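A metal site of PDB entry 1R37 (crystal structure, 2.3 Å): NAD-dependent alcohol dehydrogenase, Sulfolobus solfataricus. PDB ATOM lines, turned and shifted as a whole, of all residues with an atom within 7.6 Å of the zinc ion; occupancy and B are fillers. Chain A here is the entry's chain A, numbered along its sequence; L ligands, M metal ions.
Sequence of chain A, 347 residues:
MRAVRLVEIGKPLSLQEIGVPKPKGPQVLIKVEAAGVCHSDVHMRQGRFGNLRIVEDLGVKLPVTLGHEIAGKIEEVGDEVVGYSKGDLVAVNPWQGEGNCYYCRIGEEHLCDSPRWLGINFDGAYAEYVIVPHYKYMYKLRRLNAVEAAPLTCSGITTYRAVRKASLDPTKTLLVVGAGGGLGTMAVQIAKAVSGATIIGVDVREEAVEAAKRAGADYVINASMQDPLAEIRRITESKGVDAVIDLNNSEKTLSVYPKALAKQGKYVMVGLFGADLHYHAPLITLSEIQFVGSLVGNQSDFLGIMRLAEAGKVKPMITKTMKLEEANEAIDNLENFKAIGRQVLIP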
ATOM      1  N   GLY A  36     -16.154 -22.963 -12.826  1.00  0.00           N
ATOM      2  CA  GLY A  36     -14.803 -23.231 -13.268  1.00  0.00           C
ATOM      3  C   GLY A  36     -13.785 -22.539 -12.393  1.00  0.00           C
ATOM      4  O   GLY A  36     -14.070 -21.473 -11.835  1.00  0.00           O
ATOM      5  N   VAL A  37     -12.608 -23.142 -12.264  1.00  0.00           N
ATOM      6  CA  VAL A  37     -11.522 -22.570 -11.474  1.00  0.00           C
ATOM      7  C   VAL A  37     -10.469 -22.037 -12.439  1.00  0.00           C
ATOM      8  O   VAL A  37      -9.886 -22.791 -13.219  1.00  0.00           O
ATOM      9  CB  VAL A  37     -10.883 -23.646 -10.552  1.00  0.00           C
ATOM     10  CG1 VAL A  37      -9.738 -23.034  -9.742  1.00  0.00           C
ATOM     11  CG2 VAL A  37     -11.947 -24.234  -9.615  1.00  0.00           C
ATOM     12  N   CYS A  38     -10.229 -20.736 -12.374  1.00  0.00           N
ATOM     13  CA  CYS A  38      -9.303 -20.070 -13.267  1.00  0.00           C
ATOM     14  C   CYS A  38      -8.000 -19.694 -12.557  1.00  0.00           C
ATOM     15  O   CYS A  38      -7.999 -19.378 -11.372  1.00  0.00           O
ATOM     16  CB  CYS A  38      -9.972 -18.809 -13.801  1.00  0.00           C
ATOM     17  SG  CYS A  38      -8.998 -17.901 -15.030  1.00  0.00           S
ATOM     18  N   HIS A  39      -6.882 -19.689 -13.290  1.00  0.00           N
ATOM     19  CA  HIS A  39      -5.609 -19.343 -12.681  1.00  0.00           C
ATOM     20  C   HIS A  39      -5.640 -17.888 -12.192  1.00  0.00           C
ATOM     21  O   HIS A  39      -4.785 -17.464 -11.412  1.00  0.00           O
ATOM     22  CB  HIS A  39      -4.460 -19.560 -13.677  1.00  0.00           C
ATOM     23  CG  HIS A  39      -3.096 -19.586 -13.048  1.00  0.00           C
ATOM     24  ND1 HIS A  39      -2.248 -20.672 -13.153  1.00  0.00           N
ATOM     25  CD2 HIS A  39      -2.423 -18.653 -12.332  1.00  0.00           C
ATOM     26  CE1 HIS A  39      -1.118 -20.402 -12.526  1.00  0.00           C
ATOM     27  NE2 HIS A  39      -1.197 -19.186 -12.021  1.00  0.00           N
ATOM     28  N   SER A  40      -6.636 -17.113 -12.640  1.00  0.00           N
ATOM     29  CA  SER A  40      -6.797 -15.737 -12.161  1.00  0.00           C
ATOM     30  C   SER A  40      -7.123 -15.713 -10.677  1.00  0.00           C
ATOM     31  O   SER A  40      -6.812 -14.744  -9.974  1.00  0.00           O
ATOM     32  CB  SER A  40      -7.916 -15.016 -12.922  1.00  0.00           C
ATOM     33  OG  SER A  40      -7.516 -14.638 -14.222  1.00  0.00           O
ATOM     34  N   ASP A  41      -7.756 -16.772 -10.184  1.00  0.00           N
ATOM     35  CA  ASP A  41      -8.097 -16.856  -8.765  1.00  0.00           C
ATOM     36  C   ASP A  41      -6.851 -17.076  -7.905  1.00  0.00           C
ATOM     37  O   ASP A  41      -6.879 -16.877  -6.691  1.00  0.00           O
ATOM     38  CB  ASP A  41      -9.139 -17.954  -8.514  1.00  0.00           C
ATOM     39  CG  ASP A  41     -10.452 -17.688  -9.238  1.00  0.00           C
ATOM     40  OD1 ASP A  41     -10.882 -16.506  -9.275  1.00  0.00           O
ATOM     41  OD2 ASP A  41     -11.070 -18.642  -9.771  1.00  0.00           O
ATOM     42  N   HIS A  68     -15.644 -16.920 -11.550  1.00  0.00           N
ATOM     43  CA  HIS A  68     -16.175 -16.214 -12.702  1.00  0.00           C
ATOM     44  C   HIS A  68     -16.429 -17.065 -13.944  1.00  0.00           C
ATOM     45  O   HIS A  68     -16.654 -16.528 -15.021  1.00  0.00           O
ATOM     46  CB  HIS A  68     -15.281 -15.035 -13.064  1.00  0.00           C
ATOM     47  CG  HIS A  68     -13.840 -15.402 -13.202  1.00  0.00           C
ATOM     48  ND1 HIS A  68     -12.928 -15.382 -12.159  1.00  0.00           N
ATOM     49  CD2 HIS A  68     -13.157 -15.890 -14.276  1.00  0.00           C
ATOM     50  CE1 HIS A  68     -11.762 -15.852 -12.628  1.00  0.00           C
ATOM     51  NE2 HIS A  68     -11.855 -16.166 -13.906  1.00  0.00           N
ATOM     52  N   GLU A  69     -16.357 -18.389 -13.801  1.00  0.00           N
ATOM     53  CA  GLU A  69     -16.715 -19.281 -14.901  1.00  0.00           C
ATOM     54  C   GLU A  69     -18.033 -19.828 -14.364  1.00  0.00           C
ATOM     55  O   GLU A  69     -18.059 -20.695 -13.488  1.00  0.00           O
ATOM     56  CB  GLU A  69     -15.670 -20.385 -15.127  1.00  0.00           C
ATOM     57  CG  GLU A  69     -14.352 -19.817 -15.652  1.00  0.00           C
ATOM     58  CD  GLU A  69     -13.435 -20.837 -16.320  1.00  0.00           C
ATOM     59  OE1 GLU A  69     -13.167 -21.902 -15.721  1.00  0.00           O
ATOM     60  OE2 GLU A  69     -12.960 -20.560 -17.435  1.00  0.00           O
ATOM     61  N   TRP A  95     -18.673 -10.590 -17.248  1.00  0.00           N
ATOM     62  CA  TRP A  95     -17.986  -9.329 -17.547  1.00  0.00           C
ATOM     63  C   TRP A  95     -19.017  -8.312 -17.991  1.00  0.00           C
ATOM     64  O   TRP A  95     -19.149  -7.990 -19.173  1.00  0.00           O
ATOM     65  CB  TRP A  95     -16.951  -9.595 -18.650  1.00  0.00           C
ATOM     66  CG  TRP A  95     -16.218 -10.871 -18.405  1.00  0.00           C
ATOM     67  CD1 TRP A  95     -16.248 -12.014 -19.174  1.00  0.00           C
ATOM     68  CD2 TRP A  95     -15.380 -11.172 -17.278  1.00  0.00           C
ATOM     69  NE1 TRP A  95     -15.482 -12.999 -18.578  1.00  0.00           N
ATOM     70  CE2 TRP A  95     -14.945 -12.506 -17.418  1.00  0.00           C
ATOM     71  CE3 TRP A  95     -14.967 -10.429 -16.150  1.00  0.00           C
ATOM     72  CZ2 TRP A  95     -14.102 -13.121 -16.484  1.00  0.00           C
ATOM     73  CZ3 TRP A  95     -14.131 -11.045 -15.223  1.00  0.00           C
ATOM     74  CH2 TRP A  95     -13.712 -12.381 -15.390  1.00  0.00           C
ATOM     75  N   ILE A 120     -14.827 -11.022  -9.373  1.00  0.00           N
ATOM     76  CA  ILE A 120     -13.672 -10.143  -9.230  1.00  0.00           C
ATOM     77  C   ILE A 120     -13.983  -8.993  -8.279  1.00  0.00           C
ATOM     78  O   ILE A 120     -13.372  -8.884  -7.217  1.00  0.00           O
ATOM     79  CB  ILE A 120     -13.207  -9.582 -10.590  1.00  0.00           C
ATOM     80  CG1 ILE A 120     -13.013 -10.718 -11.604  1.00  0.00           C
ATOM     81  CG2 ILE A 120     -11.890  -8.844 -10.421  1.00  0.00           C
ATOM     82  CD1 ILE A 120     -11.915 -11.703 -11.226  1.00  0.00           C
ATOM     83  N   PRO A 151     -16.730 -23.200 -18.036  1.00  0.00           N
ATOM     84  CA  PRO A 151     -15.424 -22.726 -18.508  1.00  0.00           C
ATOM     85  C   PRO A 151     -15.480 -21.751 -19.683  1.00  0.00           C
ATOM     86  O   PRO A 151     -14.559 -20.979 -19.902  1.00  0.00           O
ATOM     87  CB  PRO A 151     -14.691 -24.019 -18.860  1.00  0.00           C
ATOM     88  CG  PRO A 151     -15.349 -25.039 -17.940  1.00  0.00           C
ATOM     89  CD  PRO A 151     -16.792 -24.668 -18.032  1.00  0.00           C
ATOM     90  N   THR A 153     -17.317 -19.202 -19.988  1.00  0.00           N
ATOM     91  CA  THR A 153     -17.566 -17.838 -19.544  1.00  0.00           C
ATOM     92  C   THR A 153     -16.312 -17.075 -19.166  1.00  0.00           C
ATOM     93  O   THR A 153     -16.376 -15.936 -18.718  1.00  0.00           O
ATOM     94  CB  THR A 153     -18.559 -17.805 -18.361  1.00  0.00           C
ATOM     95  OG1 THR A 153     -17.977 -18.431 -17.214  1.00  0.00           O
ATOM     96  CG2 THR A 153     -19.833 -18.536 -18.734  1.00  0.00           C
ATOM     97  N   CYS A 154     -15.165 -17.722 -19.336  1.00  0.00           N
ATOM     98  CA  CYS A 154     -13.890 -17.049 -19.128  1.00  0.00           C
ATOM     99  C   CYS A 154     -12.839 -17.582 -20.089  1.00  0.00           C
ATOM    100  O   CYS A 154     -12.439 -16.890 -21.016  1.00  0.00           O
ATOM    101  CB  CYS A 154     -13.374 -17.190 -17.703  1.00  0.00           C
ATOM    102  SG  CYS A 154     -11.832 -16.236 -17.539  1.00  0.00           S
ATOM    103  N   SER A 155     -12.381 -18.802 -19.851  1.00  0.00           N
ATOM    104  CA  SER A 155     -11.352 -19.392 -20.703  1.00  0.00           C
ATOM    105  C   SER A 155     -11.791 -19.449 -22.169  1.00  0.00           C
ATOM    106  O   SER A 155     -10.971 -19.257 -23.079  1.00  0.00           O
ATOM    107  CB  SER A 155     -10.988 -20.804 -20.215  1.00  0.00           C
ATOM    108  OG  SER A 155     -12.065 -21.713 -20.340  1.00  0.00           O
ATOM    109  N   THR A 158     -12.422 -15.532 -23.510  1.00  0.00           N
ATOM    110  CA  THR A 158     -11.136 -14.857 -23.545  1.00  0.00           C
ATOM    111  C   THR A 158     -10.297 -15.320 -24.726  1.00  0.00           C
ATOM    112  O   THR A 158      -9.731 -14.498 -25.459  1.00  0.00           O
ATOM    113  CB  THR A 158     -10.294 -15.122 -22.272  1.00  0.00           C
ATOM    114  OG1 THR A 158     -10.941 -14.566 -21.124  1.00  0.00           O
ATOM    115  CG2 THR A 158      -8.911 -14.502 -22.416  1.00  0.00           C
ATOM    116  N   LEU A 183      -6.715 -22.094 -20.446  1.00  0.00           N
ATOM    117  CA  LEU A 183      -6.918 -21.268 -21.636  1.00  0.00           C
ATOM    118  C   LEU A 183      -6.168 -21.841 -22.827  1.00  0.00           C
ATOM    119  O   LEU A 183      -6.659 -21.789 -23.966  1.00  0.00           O
ATOM    120  CB  LEU A 183      -6.441 -19.830 -21.383  1.00  0.00           C
ATOM    121  CG  LEU A 183      -7.459 -18.916 -20.696  1.00  0.00           C
ATOM    122  CD1 LEU A 183      -7.675 -19.394 -19.264  1.00  0.00           C
ATOM    123  CD2 LEU A 183      -6.973 -17.469 -20.716  1.00  0.00           C
ATOM    124  N   LEU A 272      -1.386 -13.373 -17.073  1.00  0.00           N
ATOM    125  CA  LEU A 272      -1.179 -12.337 -16.070  1.00  0.00           C
ATOM    126  C   LEU A 272      -0.162 -12.688 -14.994  1.00  0.00           C
ATOM    127  O   LEU A 272      -0.294 -12.272 -13.832  1.00  0.00           O
ATOM    128  CB  LEU A 272      -2.536 -11.987 -15.445  1.00  0.00           C
ATOM    129  CG  LEU A 272      -3.543 -11.341 -16.405  1.00  0.00           C
ATOM    130  CD1 LEU A 272      -4.934 -11.395 -15.797  1.00  0.00           C
ATOM    131  CD2 LEU A 272      -3.134  -9.884 -16.706  1.00  0.00           C
ATOM    132  N   VAL A 296     -10.688 -10.811 -21.341  1.00  0.00           N
ATOM    133  CA  VAL A 296     -11.927 -11.570 -21.414  1.00  0.00           C
ATOM    134  C   VAL A 296     -12.668 -11.353 -22.739  1.00  0.00           C
ATOM    135  O   VAL A 296     -12.112 -11.634 -23.790  1.00  0.00           O
ATOM    136  CB  VAL A 296     -12.831 -11.252 -20.191  1.00  0.00           C
ATOM    137  CG1 VAL A 296     -12.071 -11.656 -18.918  1.00  0.00           C
ATOM    138  CG2 VAL A 296     -13.189  -9.757 -20.125  1.00  0.00           C
ATOM    139  N   ARG A 342      -8.910 -27.948 -17.687  1.00  0.00           N
ATOM    140  CA  ARG A 342      -9.687 -27.143 -16.763  1.00  0.00           C
ATOM    141  C   ARG A 342     -10.293 -27.935 -15.602  1.00  0.00           C
ATOM    142  O   ARG A 342     -10.706 -29.083 -15.771  1.00  0.00           O
ATOM    143  CB  ARG A 342     -10.807 -26.443 -17.536  1.00  0.00           C
ATOM    144  CG  ARG A 342     -11.363 -25.190 -16.879  1.00  0.00           C
ATOM    145  CD  ARG A 342     -10.226 -24.246 -16.520  1.00  0.00           C
ATOM    146  NE  ARG A 342     -10.573 -22.837 -16.673  1.00  0.00           N
ATOM    147  CZ  ARG A 342      -9.693 -21.855 -16.556  1.00  0.00           C
ATOM    148  NH1 ARG A 342      -8.419 -22.130 -16.277  1.00  0.00           N
ATOM    149  NH2 ARG A 342     -10.074 -20.587 -16.719  1.00  0.00           N
HETATM  150  C1  LIG L   1      -9.219 -12.096 -14.743  1.00  0.00           C
HETATM  151  O1  LIG L   1      -9.033 -10.737 -15.159  1.00  0.00           O
HETATM  152  C2  LIG L   1      -8.191  -9.963 -14.302  1.00  0.00           C
HETATM  153  C3  LIG L   1      -9.036  -8.999 -13.498  1.00  0.00           C
HETATM  154  O2  LIG L   1     -10.087 -14.192 -15.543  1.00  0.00           O
HETATM  155  C4  LIG L   1     -10.142 -12.788 -15.682  1.00  0.00           C
HETATM  156  P1  LG2 L   2      -3.261 -22.756 -16.091  1.00  0.00           P
HETATM  157  O1  LG2 L   2      -4.393 -23.664 -16.398  1.00  0.00           O
HETATM  158  O2  LG2 L   2      -2.540 -22.884 -14.782  1.00  0.00           O
HETATM  159  O3  LG2 L   2      -2.259 -22.894 -17.306  1.00  0.00           O
HETATM  160  C1  LG2 L   2      -0.968 -22.194 -17.381  1.00  0.00           C
HETATM  161  C2  LG2 L   2      -0.074 -23.053 -18.235  1.00  0.00           C
HETATM  162  O4  LG2 L   2       1.223 -22.344 -18.319  1.00  0.00           O
HETATM  163  C3  LG2 L   2       0.290 -24.473 -17.640  1.00  0.00           C
HETATM  164  O5  LG2 L   2      -0.152 -25.534 -18.552  1.00  0.00           O
HETATM  165  C4  LG2 L   2       1.789 -24.448 -17.419  1.00  0.00           C
HETATM  166  O6  LG2 L   2       2.501 -25.638 -17.496  1.00  0.00           O
HETATM  167  C5  LG2 L   2       2.200 -23.364 -18.441  1.00  0.00           C
HETATM  168  N1  LG2 L   2       3.507 -22.792 -18.139  1.00  0.00           N
HETATM  169  C6  LG2 L   2       4.148 -22.438 -16.949  1.00  0.00           C
HETATM  170  N2  LG2 L   2       5.368 -21.941 -17.138  1.00  0.00           N
HETATM  171  C7  LG2 L   2       5.593 -21.934 -18.461  1.00  0.00           C
HETATM  172  C8  LG2 L   2       6.737 -21.508 -19.293  1.00  0.00           C
HETATM  173  N3  LG2 L   2       7.858 -21.019 -18.782  1.00  0.00           N
HETATM  174  N4  LG2 L   2       6.564 -21.679 -20.659  1.00  0.00           N
HETATM  175  C9  LG2 L   2       5.466 -22.177 -21.243  1.00  0.00           C
HETATM  176  N5  LG2 L   2       4.351 -22.594 -20.507  1.00  0.00           N
HETATM  177  C10 LG2 L   2       4.454 -22.459 -19.117  1.00  0.00           C
HETATM  178  O7  LG2 L   2      -3.756 -21.266 -16.171  1.00  0.00           O
HETATM  179  P2  LG2 L   2      -4.957 -20.539 -16.991  1.00  0.00           P
HETATM  180  O8  LG2 L   2      -6.204 -20.640 -16.237  1.00  0.00           O
HETATM  181  O9  LG2 L   2      -4.895 -21.111 -18.380  1.00  0.00           O
HETATM  182  O10 LG2 L   2      -4.467 -18.997 -16.886  1.00  0.00           O
HETATM  183  C11 LG2 L   2      -3.215 -18.541 -17.522  1.00  0.00           C
HETATM  184  C12 LG2 L   2      -3.053 -17.080 -17.305  1.00  0.00           C
HETATM  185  O11 LG2 L   2      -4.160 -16.382 -18.000  1.00  0.00           O
HETATM  186  C13 LG2 L   2      -3.166 -16.595 -15.803  1.00  0.00           C
HETATM  187  O12 LG2 L   2      -2.138 -15.634 -15.487  1.00  0.00           O
HETATM  188  C14 LG2 L   2      -4.561 -15.945 -15.729  1.00  0.00           C
HETATM  189  O13 LG2 L   2      -4.723 -15.018 -14.686  1.00  0.00           O
HETATM  190  C15 LG2 L   2      -4.689 -15.331 -17.172  1.00  0.00           C
HETATM  191  N6  LG2 L   2      -6.071 -15.087 -17.661  1.00  0.00           N
HETATM  192  C16 LG2 L   2      -6.296 -13.878 -18.400  1.00  0.00           C
HETATM  193  C17 LG2 L   2      -7.492 -13.558 -18.896  1.00  0.00           C
HETATM  194  C18 LG2 L   2      -7.696 -12.273 -19.681  1.00  0.00           C
HETATM  195  O14 LG2 L   2      -8.849 -11.832 -19.809  1.00  0.00           O
HETATM  196  N7  LG2 L   2      -6.632 -11.651 -20.222  1.00  0.00           N
HETATM  197  C19 LG2 L   2      -8.731 -14.448 -18.711  1.00  0.00           C
HETATM  198  C20 LG2 L   2      -8.455 -15.722 -17.919  1.00  0.00           C
HETATM  199  C21 LG2 L   2      -7.144 -15.994 -17.422  1.00  0.00           C
HETATM  200 ZN    ZN M   1     -10.626 -16.380 -15.579  1.00  0.00          ZN
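OG of Ser 40 touches the zinc ion (3.8 Å).
Within 4 Å of the zinc ion: Cys 38, Ser 40, His 68 and Cys 154.
The nearest printed residue that does not touch the zinc ion is Arg 342 (4.4 Å).
O of His 68 lies within hydrogen-bond range of OG1 of Thr 153, 3.2 Å away.
The side-chain sulfur (SG) of Cys 38 lies close to the backbone NH (N) of Ser 40 (3.5 Å).
The guanidinium group of Arg 342 sits close to the side-chain sulfur of Cys 38.
The side-chain carboxylate (OD2) of Asp 41 lies within hydrogen-bond range of the backbone NH (N) of Cys 38.
O of Cys 154 sits at hydrogen-bond distance from OG1 of Thr 158 (2.8 Å).
O13 of LG2 L2 sits close to N of Ser 40.
The side-chain hydroxyl (OG) of Ser 40 lies within hydrogen-bond range of an oxygen (O13) of LG2 L2, 2.9 Å away.
O8 of LG2 L2 lies within salt-bridge range of NH1 of Arg 342.
The backbone NH (N) of His 39 lies within hydrogen-bond range of an oxygen (O8) of LG2 L2 (3.2 Å).
ND1 of His 39 sits at hydrogen-bond distance from O2 of LG2 L2 (2.8 Å).
An oxygen (O9) of LG2 L2 sits at hydrogen-bond distance from the backbone NH (N) of Leu 183, 2.9 Å away.
The backbone NH (N) of Val 296 sits at hydrogen-bond distance from an oxygen (O14) of LG2 L2, 2.6 Å away.
N of Leu 272 lies within hydrogen-bond range of O12 of LG2 L2 (2.9 Å).
The zinc ion is bound by a ring nitrogen (NE2) of His 68 (2.1 Å), an oxygen (O2) of LIG L1 (2.3 Å), the side-chain sulfur (SG) of Cys 38 (2.3 Å) and the side-chain sulfur (SG) of Cys 154 (2.3 Å).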
